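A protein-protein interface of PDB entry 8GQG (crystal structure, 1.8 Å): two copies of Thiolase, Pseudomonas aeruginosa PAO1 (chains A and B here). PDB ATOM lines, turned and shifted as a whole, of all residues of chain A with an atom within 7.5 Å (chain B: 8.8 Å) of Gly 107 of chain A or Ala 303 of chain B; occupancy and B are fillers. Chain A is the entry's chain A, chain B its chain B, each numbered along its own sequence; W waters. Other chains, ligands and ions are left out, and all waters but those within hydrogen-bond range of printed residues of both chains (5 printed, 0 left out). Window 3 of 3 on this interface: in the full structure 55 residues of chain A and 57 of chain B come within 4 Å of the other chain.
The side-chain amide nitrogen (ND2) of Asn 102 of chain B lies within hydrogen-bond range of the side-chain amide oxygen (OE1) of Gln 103 of chain A (3.2 Å). O of Phe 279 of chain B lies within hydrogen-bond range of NE2 of Gln 103 of chain A (2.9 Å).
Of the 18 printed residues of chain B, 6 touch a printed residue of chain A. Of the 11 printed residues of chain A, 5 touch a printed residue of chain B.
Gly 107 of chain A touches just one residue of chain B: Ala 303 (3.9 Å). Of the printed residues of chain A, Ala 303 of chain B touches Gly 107. Of the printed residues of chain A, Gly 278 of chain B touches Cys 108 (3.8 Å). Printed residues of chain A within 4 Å of Lys 304 of chain B: Cys 108. Lys 299 of chain B touches none of the printed residues of chain A. The nearest residue of chain A that does not touch Ala 303 of chain B is Cys 108 of chain A (4.1 Å). The nearest printed residue of chain B that does not touch Asn 102 of chain A is Phe 276 of chain B (7.6 Å).
Water W1 lies within hydrogen-bond range of the side-chain amide oxygen (OE1) of Gln 103 of chain A (2.8 Å) and the side-chain amide nitrogen (ND2) of Asn 102 of chain B (3.0 Å). Water W2 lies within hydrogen-bond range of NZ of Lys 304 of chain B (2.8 Å), O of Ser 106 of chain A (2.9 Å), O of Arg 277 of chain B (3.2 Å) and SG of Cys 108 of chain A (3.4 Å). Water W5 lies within hydrogen-bond range of O of Gly 107 of chain A (2.9 Å) and O of Ala 303 of chain B (3.5 Å). Water W4 lies within hydrogen-bond range of the side-chain amide oxygen (OE1) of Gln 103 of chain A (3.0 Å), the side-chain hydroxyl (OG) of Ser 106 of chain A (3.0 Å), the side-chain amide nitrogen (ND2) of Asn 102 of chain B (3.0 Å) and the backbone NH (N) of Phe 279 of chain B (3.1 Å). Water W3 bridges the backbone carbonyl oxygen of Asn 102 of chain A (3.1 Å) and the backbone carbonyl oxygen of Asn 102 of chain B (3.1 Å).
O of Asn 102 of chain B touches CB of Asn 102 of chain A (3.7 Å). CB of Ser 106 of chain A touches OD1 of Asn 102 of chain B, 3.4 Å away. Gly 107 of chain A touches Ala 303 of chain B. Cys 108 of chain A touches Gly 278 of chain B (SG to CA, 3.8 Å). Cys 108 of chain A touches Phe 279 of chain B (CB to O, 3.2 Å). O of Cys 108 of chain A touches CG2 of Thr 280 of chain B (3.7 Å). SG of Cys 108 of chain A touches CD of Lys 304 of chain B, 3.97 Å away.
O of Gln 103 of chain A sits at hydrogen-bond distance from OG of Ser 106 of chain A (2.6 Å). NE2 of Gln 103 of chain A is in hydrogen-bond range of OG of Ser 109 of chain A. The side-chain amino group (NZ) of Lys 304 of chain B lies close to the backbone carbonyl oxygen (O) of Arg 277 of chain B (3.1 Å). The backbone carbonyl oxygen (O) of Gly 278 of chain B is in hydrogen-bond range of the backbone NH (N) of Leu 389 of chain B (2.8 Å). OG of Ser 106 of chain A is in hydrogen-bond range of N of Cys 108 of chain A (3.2 Å). The side-chain hydroxyl (OG1) of Thr 280 of chain B sits at hydrogen-bond distance from the backbone carbonyl oxygen (O) of Ser 296 of chain B.
Asn 102 of chain A touches its own counterpart, Asn 102 of chain B. Position printed for both chains: 102. Of the 9 pairs that touch across the chains among the printed residues, 1 has its exchanged pair printed and touching as well.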
ATOM      1  N   ARG A   2      25.524  -5.425 -15.979  1.00  0.00           N
ATOM      2  CA  ARG A   2      26.215  -5.206 -14.678  1.00  0.00           C
ATOM      3  C   ARG A   2      25.401  -5.880 -13.562  1.00  0.00           C
ATOM      4  O   ARG A   2      24.264  -5.455 -13.277  1.00  0.00           O
ATOM      5  CB  ARG A   2      26.401  -3.714 -14.408  1.00  0.00           C
ATOM      6  CG  ARG A   2      27.238  -3.408 -13.175  1.00  0.00           C
ATOM      7  CD  ARG A   2      27.600  -1.938 -13.212  1.00  0.00           C
ATOM      8  NE  ARG A   2      28.220  -1.395 -12.021  1.00  0.00           N
ATOM      9  CZ  ARG A   2      29.432  -1.713 -11.603  1.00  0.00           C
ATOM     10  NH1 ARG A   2      30.161  -2.632 -12.219  1.00  0.00           N
ATOM     11  NH2 ARG A   2      29.901  -1.128 -10.526  1.00  0.00           N
ATOM     12  N   ALA A 101      19.064  -1.094  -7.257  1.00  0.00           N
ATOM     13  CA  ALA A 101      19.708  -2.131  -8.108  1.00  0.00           C
ATOM     14  C   ALA A 101      19.872  -1.580  -9.526  1.00  0.00           C
ATOM     15  O   ALA A 101      20.972  -1.675 -10.099  1.00  0.00           O
ATOM     16  CB  ALA A 101      18.897  -3.412  -8.057  1.00  0.00           C
ATOM     17  N   ASN A 102      18.863  -0.909 -10.063  1.00  0.00           N
ATOM     18  CA  ASN A 102      18.908  -0.384 -11.448  1.00  0.00           C
ATOM     19  C   ASN A 102      19.886   0.790 -11.510  1.00  0.00           C
ATOM     20  O   ASN A 102      20.541   0.948 -12.538  1.00  0.00           O
ATOM     21  CB  ASN A 102      17.506  -0.091 -11.951  1.00  0.00           C
ATOM     22  CG  ASN A 102      16.715  -1.352 -12.232  1.00  0.00           C
ATOM     23  OD1 ASN A 102      17.272  -2.335 -12.699  1.00  0.00           O
ATOM     24  ND2 ASN A 102      15.425  -1.309 -12.001  1.00  0.00           N
ATOM     25  N   GLN A 103      19.974   1.602 -10.459  1.00  0.00           N
ATOM     26  CA  GLN A 103      20.958   2.712 -10.383  1.00  0.00           C
ATOM     27  C   GLN A 103      22.379   2.113 -10.420  1.00  0.00           C
ATOM     28  O   GLN A 103      23.257   2.697 -11.085  1.00  0.00           O
ATOM     29  CB  GLN A 103      20.741   3.543  -9.104  1.00  0.00           C
ATOM     30  CG  GLN A 103      21.808   4.597  -8.821  1.00  0.00           C
ATOM     31  CD  GLN A 103      21.967   5.637  -9.917  1.00  0.00           C
ATOM     32  OE1 GLN A 103      21.111   5.838 -10.790  1.00  0.00           O
ATOM     33  NE2 GLN A 103      23.077   6.350  -9.849  1.00  0.00           N
ATOM     34  N   ILE A 104      22.654   1.084  -9.614  1.00  0.00           N
ATOM     35  CA  ILE A 104      24.016   0.469  -9.585  1.00  0.00           C
ATOM     36  C   ILE A 104      24.269  -0.175 -10.946  1.00  0.00           C
ATOM     37  O   ILE A 104      25.385  -0.042 -11.465  1.00  0.00           O
ATOM     38  CB  ILE A 104      24.150  -0.538  -8.433  1.00  0.00           C
ATOM     39  CG1 ILE A 104      24.126   0.170  -7.082  1.00  0.00           C
ATOM     40  CG2 ILE A 104      25.395  -1.430  -8.574  1.00  0.00           C
ATOM     41  CD1 ILE A 104      23.924  -0.791  -5.964  1.00  0.00           C
ATOM     42  N   ALA A 105      23.257  -0.814 -11.514  1.00  0.00           N
ATOM     43  CA  ALA A 105      23.394  -1.509 -12.813  1.00  0.00           C
ATOM     44  C   ALA A 105      23.794  -0.503 -13.893  1.00  0.00           C
ATOM     45  O   ALA A 105      24.450  -0.914 -14.861  1.00  0.00           O
ATOM     46  CB  ALA A 105      22.122  -2.202 -13.170  1.00  0.00           C
ATOM     47  N   SER A 106      23.421   0.772 -13.749  1.00  0.00           N
ATOM     48  CA  SER A 106      23.704   1.817 -14.768  1.00  0.00           C
ATOM     49  C   SER A 106      25.191   2.131 -14.773  1.00  0.00           C
ATOM     50  O   SER A 106      25.599   2.800 -15.716  1.00  0.00           O
ATOM     51  CB  SER A 106      22.934   3.111 -14.522  1.00  0.00           C
ATOM     52  OG  SER A 106      23.521   3.807 -13.443  1.00  0.00           O
ATOM     53  N   GLY A 107      25.934   1.754 -13.735  1.00  0.00           N
ATOM     54  CA  GLY A 107      27.372   2.056 -13.568  1.00  0.00           C
ATOM     55  C   GLY A 107      27.612   3.376 -12.854  1.00  0.00           C
ATOM     56  O   GLY A 107      28.766   3.734 -12.676  1.00  0.00           O
ATOM     57  N   CYS A 108      26.581   4.086 -12.385  1.00  0.00           N
ATOM     58  CA  CYS A 108      26.800   5.432 -11.771  1.00  0.00           C
ATOM     59  C   CYS A 108      26.815   5.379 -10.239  1.00  0.00           C
ATOM     60  O   CYS A 108      27.000   6.438  -9.604  1.00  0.00           O
ATOM     61  CB  CYS A 108      25.748   6.394 -12.288  1.00  0.00           C
ATOM     62  SG  CYS A 108      25.952   6.765 -14.056  1.00  0.00           S
ATOM     63  N   SER A 109      26.608   4.207  -9.656  1.00  0.00           N
ATOM     64  CA  SER A 109      26.744   3.950  -8.202  1.00  0.00           C
ATOM     65  C   SER A 109      27.307   2.538  -8.019  1.00  0.00           C
ATOM     66  O   SER A 109      27.090   1.714  -8.930  1.00  0.00           O
ATOM     67  CB  SER A 109      25.413   4.078  -7.461  1.00  0.00           C
ATOM     68  OG  SER A 109      24.883   5.386  -7.588  1.00  0.00           O
ATOM     69  N   GLU A 110      27.899   2.283  -6.853  1.00  0.00           N
ATOM     70  CA  GLU A 110      28.484   0.978  -6.465  1.00  0.00           C
ATOM     71  C   GLU A 110      27.711   0.367  -5.298  1.00  0.00           C
ATOM     72  O   GLU A 110      27.614  -0.868  -5.268  1.00  0.00           O
ATOM     73  CB  GLU A 110      29.964   1.164  -6.086  1.00  0.00           C
ATOM     74  CG  GLU A 110      30.890   1.540  -7.242  1.00  0.00           C
ATOM     75  CD  GLU A 110      30.719   0.660  -8.471  1.00  0.00           C
ATOM     76  OE1 GLU A 110      30.747  -0.592  -8.330  1.00  0.00           O
ATOM     77  OE2 GLU A 110      30.499   1.212  -9.558  1.00  0.00           O
ATOM     78  N   ASN B 102      16.549   3.964 -16.040  1.00  0.00           N
ATOM     79  CA  ASN B 102      17.222   2.776 -15.444  1.00  0.00           C
ATOM     80  C   ASN B 102      16.240   1.596 -15.379  1.00  0.00           C
ATOM     81  O   ASN B 102      16.702   0.450 -15.548  1.00  0.00           O
ATOM     82  CB  ASN B 102      17.890   3.117 -14.112  1.00  0.00           C
ATOM     83  CG  ASN B 102      19.076   4.038 -14.304  1.00  0.00           C
ATOM     84  OD1 ASN B 102      19.782   3.980 -15.314  1.00  0.00           O
ATOM     85  ND2 ASN B 102      19.351   4.862 -13.327  1.00  0.00           N
ATOM     86  N   PHE B 276      19.441   9.175 -22.455  1.00  0.00           N
ATOM     87  CA  PHE B 276      19.817   9.224 -21.025  1.00  0.00           C
ATOM     88  C   PHE B 276      21.150   8.522 -20.833  1.00  0.00           C
ATOM     89  O   PHE B 276      21.213   7.307 -21.173  1.00  0.00           O
ATOM     90  CB  PHE B 276      18.818   8.486 -20.154  1.00  0.00           C
ATOM     91  CG  PHE B 276      19.248   8.394 -18.718  1.00  0.00           C
ATOM     92  CD1 PHE B 276      19.088   9.473 -17.867  1.00  0.00           C
ATOM     93  CD2 PHE B 276      19.756   7.215 -18.203  1.00  0.00           C
ATOM     94  CE1 PHE B 276      19.460   9.378 -16.539  1.00  0.00           C
ATOM     95  CE2 PHE B 276      20.121   7.122 -16.869  1.00  0.00           C
ATOM     96  CZ  PHE B 276      19.961   8.204 -16.034  1.00  0.00           C
ATOM     97  N   ARG B 277      22.144   9.205 -20.279  1.00  0.00           N
ATOM     98  CA  ARG B 277      23.507   8.636 -20.140  1.00  0.00           C
ATOM     99  C   ARG B 277      23.962   8.558 -18.680  1.00  0.00           C
ATOM    100  O   ARG B 277      25.112   8.149 -18.447  1.00  0.00           O
ATOM    101  CB  ARG B 277      24.546   9.414 -20.955  1.00  0.00           C
ATOM    102  CG  ARG B 277      24.310   9.316 -22.456  1.00  0.00           C
ATOM    103  CD  ARG B 277      24.441   7.875 -22.923  1.00  0.00           C
ATOM    104  NE  ARG B 277      24.610   7.899 -24.363  1.00  0.00           N
ATOM    105  CZ  ARG B 277      24.312   6.898 -25.187  1.00  0.00           C
ATOM    106  NH1 ARG B 277      23.787   5.775 -24.728  1.00  0.00           N
ATOM    107  NH2 ARG B 277      24.547   7.033 -26.485  1.00  0.00           N
ATOM    108  N   GLY B 278      23.094   8.795 -17.716  1.00  0.00           N
ATOM    109  CA  GLY B 278      23.474   8.462 -16.338  1.00  0.00           C
ATOM    110  C   GLY B 278      23.067   9.565 -15.395  1.00  0.00           C
ATOM    111  O   GLY B 278      22.814  10.705 -15.843  1.00  0.00           O
ATOM    112  N   PHE B 279      23.023   9.209 -14.126  1.00  0.00           N
ATOM    113  CA  PHE B 279      22.603  10.084 -13.020  1.00  0.00           C
ATOM    114  C   PHE B 279      23.449   9.806 -11.783  1.00  0.00           C
ATOM    115  O   PHE B 279      23.650   8.640 -11.463  1.00  0.00           O
ATOM    116  CB  PHE B 279      21.118   9.847 -12.776  1.00  0.00           C
ATOM    117  CG  PHE B 279      20.537  10.540 -11.569  1.00  0.00           C
ATOM    118  CD1 PHE B 279      20.092  11.847 -11.653  1.00  0.00           C
ATOM    119  CD2 PHE B 279      20.331   9.844 -10.388  1.00  0.00           C
ATOM    120  CE1 PHE B 279      19.503  12.453 -10.552  1.00  0.00           C
ATOM    121  CE2 PHE B 279      19.706  10.445  -9.303  1.00  0.00           C
ATOM    122  CZ  PHE B 279      19.323  11.766  -9.391  1.00  0.00           C
ATOM    123  N   THR B 280      23.829  10.851 -11.048  1.00  0.00           N
ATOM    124  CA  THR B 280      24.472  10.749  -9.729  1.00  0.00           C
ATOM    125  C   THR B 280      23.866  11.706  -8.708  1.00  0.00           C
ATOM    126  O   THR B 280      23.231  12.697  -9.111  1.00  0.00           O
ATOM    127  CB  THR B 280      25.962  11.057  -9.842  1.00  0.00           C
ATOM    128  OG1 THR B 280      26.130  12.372 -10.385  1.00  0.00           O
ATOM    129  CG2 THR B 280      26.640   9.994 -10.676  1.00  0.00           C
ATOM    130  N   SER B 296      28.342  16.254  -6.955  1.00  0.00           N
ATOM    131  CA  SER B 296      27.617  15.266  -7.810  1.00  0.00           C
ATOM    132  C   SER B 296      28.134  15.316  -9.251  1.00  0.00           C
ATOM    133  O   SER B 296      28.164  14.254  -9.931  1.00  0.00           O
ATOM    134  CB  SER B 296      26.109  15.401  -7.704  1.00  0.00           C
ATOM    135  OG  SER B 296      25.628  16.612  -8.264  1.00  0.00           O
ATOM    136  N   VAL B 297      28.530  16.482  -9.752  1.00  0.00           N
ATOM    137  CA  VAL B 297      28.920  16.591 -11.183  1.00  0.00           C
ATOM    138  C   VAL B 297      30.192  15.753 -11.415  1.00  0.00           C
ATOM    139  O   VAL B 297      30.245  14.971 -12.368  1.00  0.00           O
ATOM    140  CB  VAL B 297      29.063  18.053 -11.635  1.00  0.00           C
ATOM    141  CG1 VAL B 297      29.873  18.182 -12.907  1.00  0.00           C
ATOM    142  CG2 VAL B 297      27.682  18.687 -11.843  1.00  0.00           C
ATOM    143  N   PRO B 298      31.244  15.894 -10.587  1.00  0.00           N
ATOM    144  CA  PRO B 298      32.511  15.168 -10.848  1.00  0.00           C
ATOM    145  C   PRO B 298      32.265  13.652 -10.783  1.00  0.00           C
ATOM    146  O   PRO B 298      32.746  12.968 -11.649  1.00  0.00           O
ATOM    147  CB  PRO B 298      33.465  15.661  -9.738  1.00  0.00           C
ATOM    148  CG  PRO B 298      32.864  16.999  -9.344  1.00  0.00           C
ATOM    149  CD  PRO B 298      31.355  16.780  -9.419  1.00  0.00           C
ATOM    150  N   LYS B 299      31.432  13.183  -9.834  1.00  0.00           N
ATOM    151  CA  LYS B 299      31.035  11.754  -9.793  1.00  0.00           C
ATOM    152  C   LYS B 299      30.442  11.331 -11.132  1.00  0.00           C
ATOM    153  O   LYS B 299      30.741  10.193 -11.568  1.00  0.00           O
ATOM    154  CB  LYS B 299      30.024  11.447  -8.695  1.00  0.00           C
ATOM    155  CG  LYS B 299      30.543  11.416  -7.277  1.00  0.00           C
ATOM    156  CD  LYS B 299      29.368  11.242  -6.322  1.00  0.00           C
ATOM    157  CE  LYS B 299      29.752  10.703  -4.971  1.00  0.00           C
ATOM    158  NZ  LYS B 299      30.977  11.354  -4.467  1.00  0.00           N
ATOM    159  N   LEU B 300      29.575  12.142 -11.751  1.00  0.00           N
ATOM    160  CA  LEU B 300      28.867  11.725 -12.973  1.00  0.00           C
ATOM    161  C   LEU B 300      29.859  11.678 -14.145  1.00  0.00           C
ATOM    162  O   LEU B 300      29.768  10.777 -15.003  1.00  0.00           O
ATOM    163  CB  LEU B 300      27.756  12.738 -13.295  1.00  0.00           C
ATOM    164  CG  LEU B 300      27.084  12.587 -14.650  1.00  0.00           C
ATOM    165  CD1 LEU B 300      26.366  11.268 -14.772  1.00  0.00           C
ATOM    166  CD2 LEU B 300      26.133  13.775 -14.948  1.00  0.00           C
ATOM    167  N   LEU B 301      30.699  12.694 -14.259  1.00  0.00           N
ATOM    168  CA  LEU B 301      31.633  12.797 -15.412  1.00  0.00           C
ATOM    169  C   LEU B 301      32.655  11.629 -15.364  1.00  0.00           C
ATOM    170  O   LEU B 301      33.000  11.103 -16.442  1.00  0.00           O
ATOM    171  CB  LEU B 301      32.334  14.154 -15.329  1.00  0.00           C
ATOM    172  CG  LEU B 301      31.428  15.373 -15.544  1.00  0.00           C
ATOM    173  CD1 LEU B 301      32.272  16.628 -15.662  1.00  0.00           C
ATOM    174  CD2 LEU B 301      30.520  15.179 -16.761  1.00  0.00           C
ATOM    175  N   LYS B 302      33.123  11.286 -14.166  1.00  0.00           N
ATOM    176  CA  LYS B 302      34.073  10.172 -13.933  1.00  0.00           C
ATOM    177  C   LYS B 302      33.379   8.857 -14.301  1.00  0.00           C
ATOM    178  O   LYS B 302      33.940   8.121 -15.120  1.00  0.00           O
ATOM    179  CB  LYS B 302      34.551  10.193 -12.491  1.00  0.00           C
ATOM    180  CG  LYS B 302      35.747   9.301 -12.189  1.00  0.00           C
ATOM    181  CD  LYS B 302      36.117   9.370 -10.724  1.00  0.00           C
ATOM    182  CE  LYS B 302      37.556   8.990 -10.433  1.00  0.00           C
ATOM    183  NZ  LYS B 302      37.736   7.521 -10.500  1.00  0.00           N
ATOM    184  N   ALA B 303      32.166   8.610 -13.792  1.00  0.00           N
ATOM    185  CA  ALA B 303      31.400   7.387 -14.105  1.00  0.00           C
ATOM    186  C   ALA B 303      31.271   7.267 -15.614  1.00  0.00           C
ATOM    187  O   ALA B 303      31.195   6.137 -16.100  1.00  0.00           O
ATOM    188  CB  ALA B 303      30.043   7.390 -13.447  1.00  0.00           C
ATOM    189  N   LYS B 304      31.217   8.374 -16.352  1.00  0.00           N
ATOM    190  CA  LYS B 304      30.885   8.324 -17.797  1.00  0.00           C
ATOM    191  C   LYS B 304      32.100   8.611 -18.681  1.00  0.00           C
ATOM    192  O   LYS B 304      31.889   8.640 -19.865  1.00  0.00           O
ATOM    193  CB  LYS B 304      29.723   9.268 -18.108  1.00  0.00           C
ATOM    194  CG  LYS B 304      28.464   8.955 -17.312  1.00  0.00           C
ATOM    195  CD  LYS B 304      28.018   7.514 -17.362  1.00  0.00           C
ATOM    196  CE  LYS B 304      27.804   6.972 -18.755  1.00  0.00           C
ATOM    197  NZ  LYS B 304      27.024   5.710 -18.703  1.00  0.00           N
ATOM    198  N   GLY B 305      33.283   8.864 -18.115  1.00  0.00           N
ATOM    199  CA  GLY B 305      34.513   9.082 -18.906  1.00  0.00           C
ATOM    200  C   GLY B 305      34.534  10.413 -19.625  1.00  0.00           C
ATOM    201  O   GLY B 305      35.019  10.442 -20.767  1.00  0.00           O
ATOM    202  N   LEU B 306      34.004  11.491 -19.019  1.00  0.00           N
ATOM    203  CA  LEU B 306      34.001  12.837 -19.658  1.00  0.00           C
ATOM    204  C   LEU B 306      34.734  13.779 -18.736  1.00  0.00           C
ATOM    205  O   LEU B 306      34.961  13.425 -17.565  1.00  0.00           O
ATOM    206  CB  LEU B 306      32.587  13.360 -19.946  1.00  0.00           C
ATOM    207  CG  LEU B 306      31.761  12.575 -20.959  1.00  0.00           C
ATOM    208  CD1 LEU B 306      30.386  13.218 -21.129  1.00  0.00           C
ATOM    209  CD2 LEU B 306      32.473  12.491 -22.307  1.00  0.00           C
ATOM    210  N   LEU B 389      23.253  13.167 -17.124  1.00  0.00           N
ATOM    211  CA  LEU B 389      23.962  13.361 -18.401  1.00  0.00           C
ATOM    212  C   LEU B 389      23.057  12.897 -19.523  1.00  0.00           C
ATOM    213  O   LEU B 389      22.487  11.814 -19.445  1.00  0.00           O
ATOM    214  CB  LEU B 389      25.275  12.566 -18.385  1.00  0.00           C
ATOM    215  CG  LEU B 389      26.069  12.630 -19.685  1.00  0.00           C
ATOM    216  CD1 LEU B 389      26.634  14.020 -19.921  1.00  0.00           C
ATOM    217  CD2 LEU B 389      27.201  11.605 -19.628  1.00  0.00           C
HETATM  218  O   HOH W   1      18.364   5.966 -10.727  1.00  0.00           O
HETATM  219  O   HOH W   2      24.907   5.303 -16.986  1.00  0.00           O
HETATM  220  O   HOH W   3      19.723  -0.199 -15.262  1.00  0.00           O
HETATM  221  O   HOH W   4      21.966   6.373 -13.573  1.00  0.00           O
HETATM  222  O   HOH W   5      31.473   3.645 -13.695  1.00  0.00           O
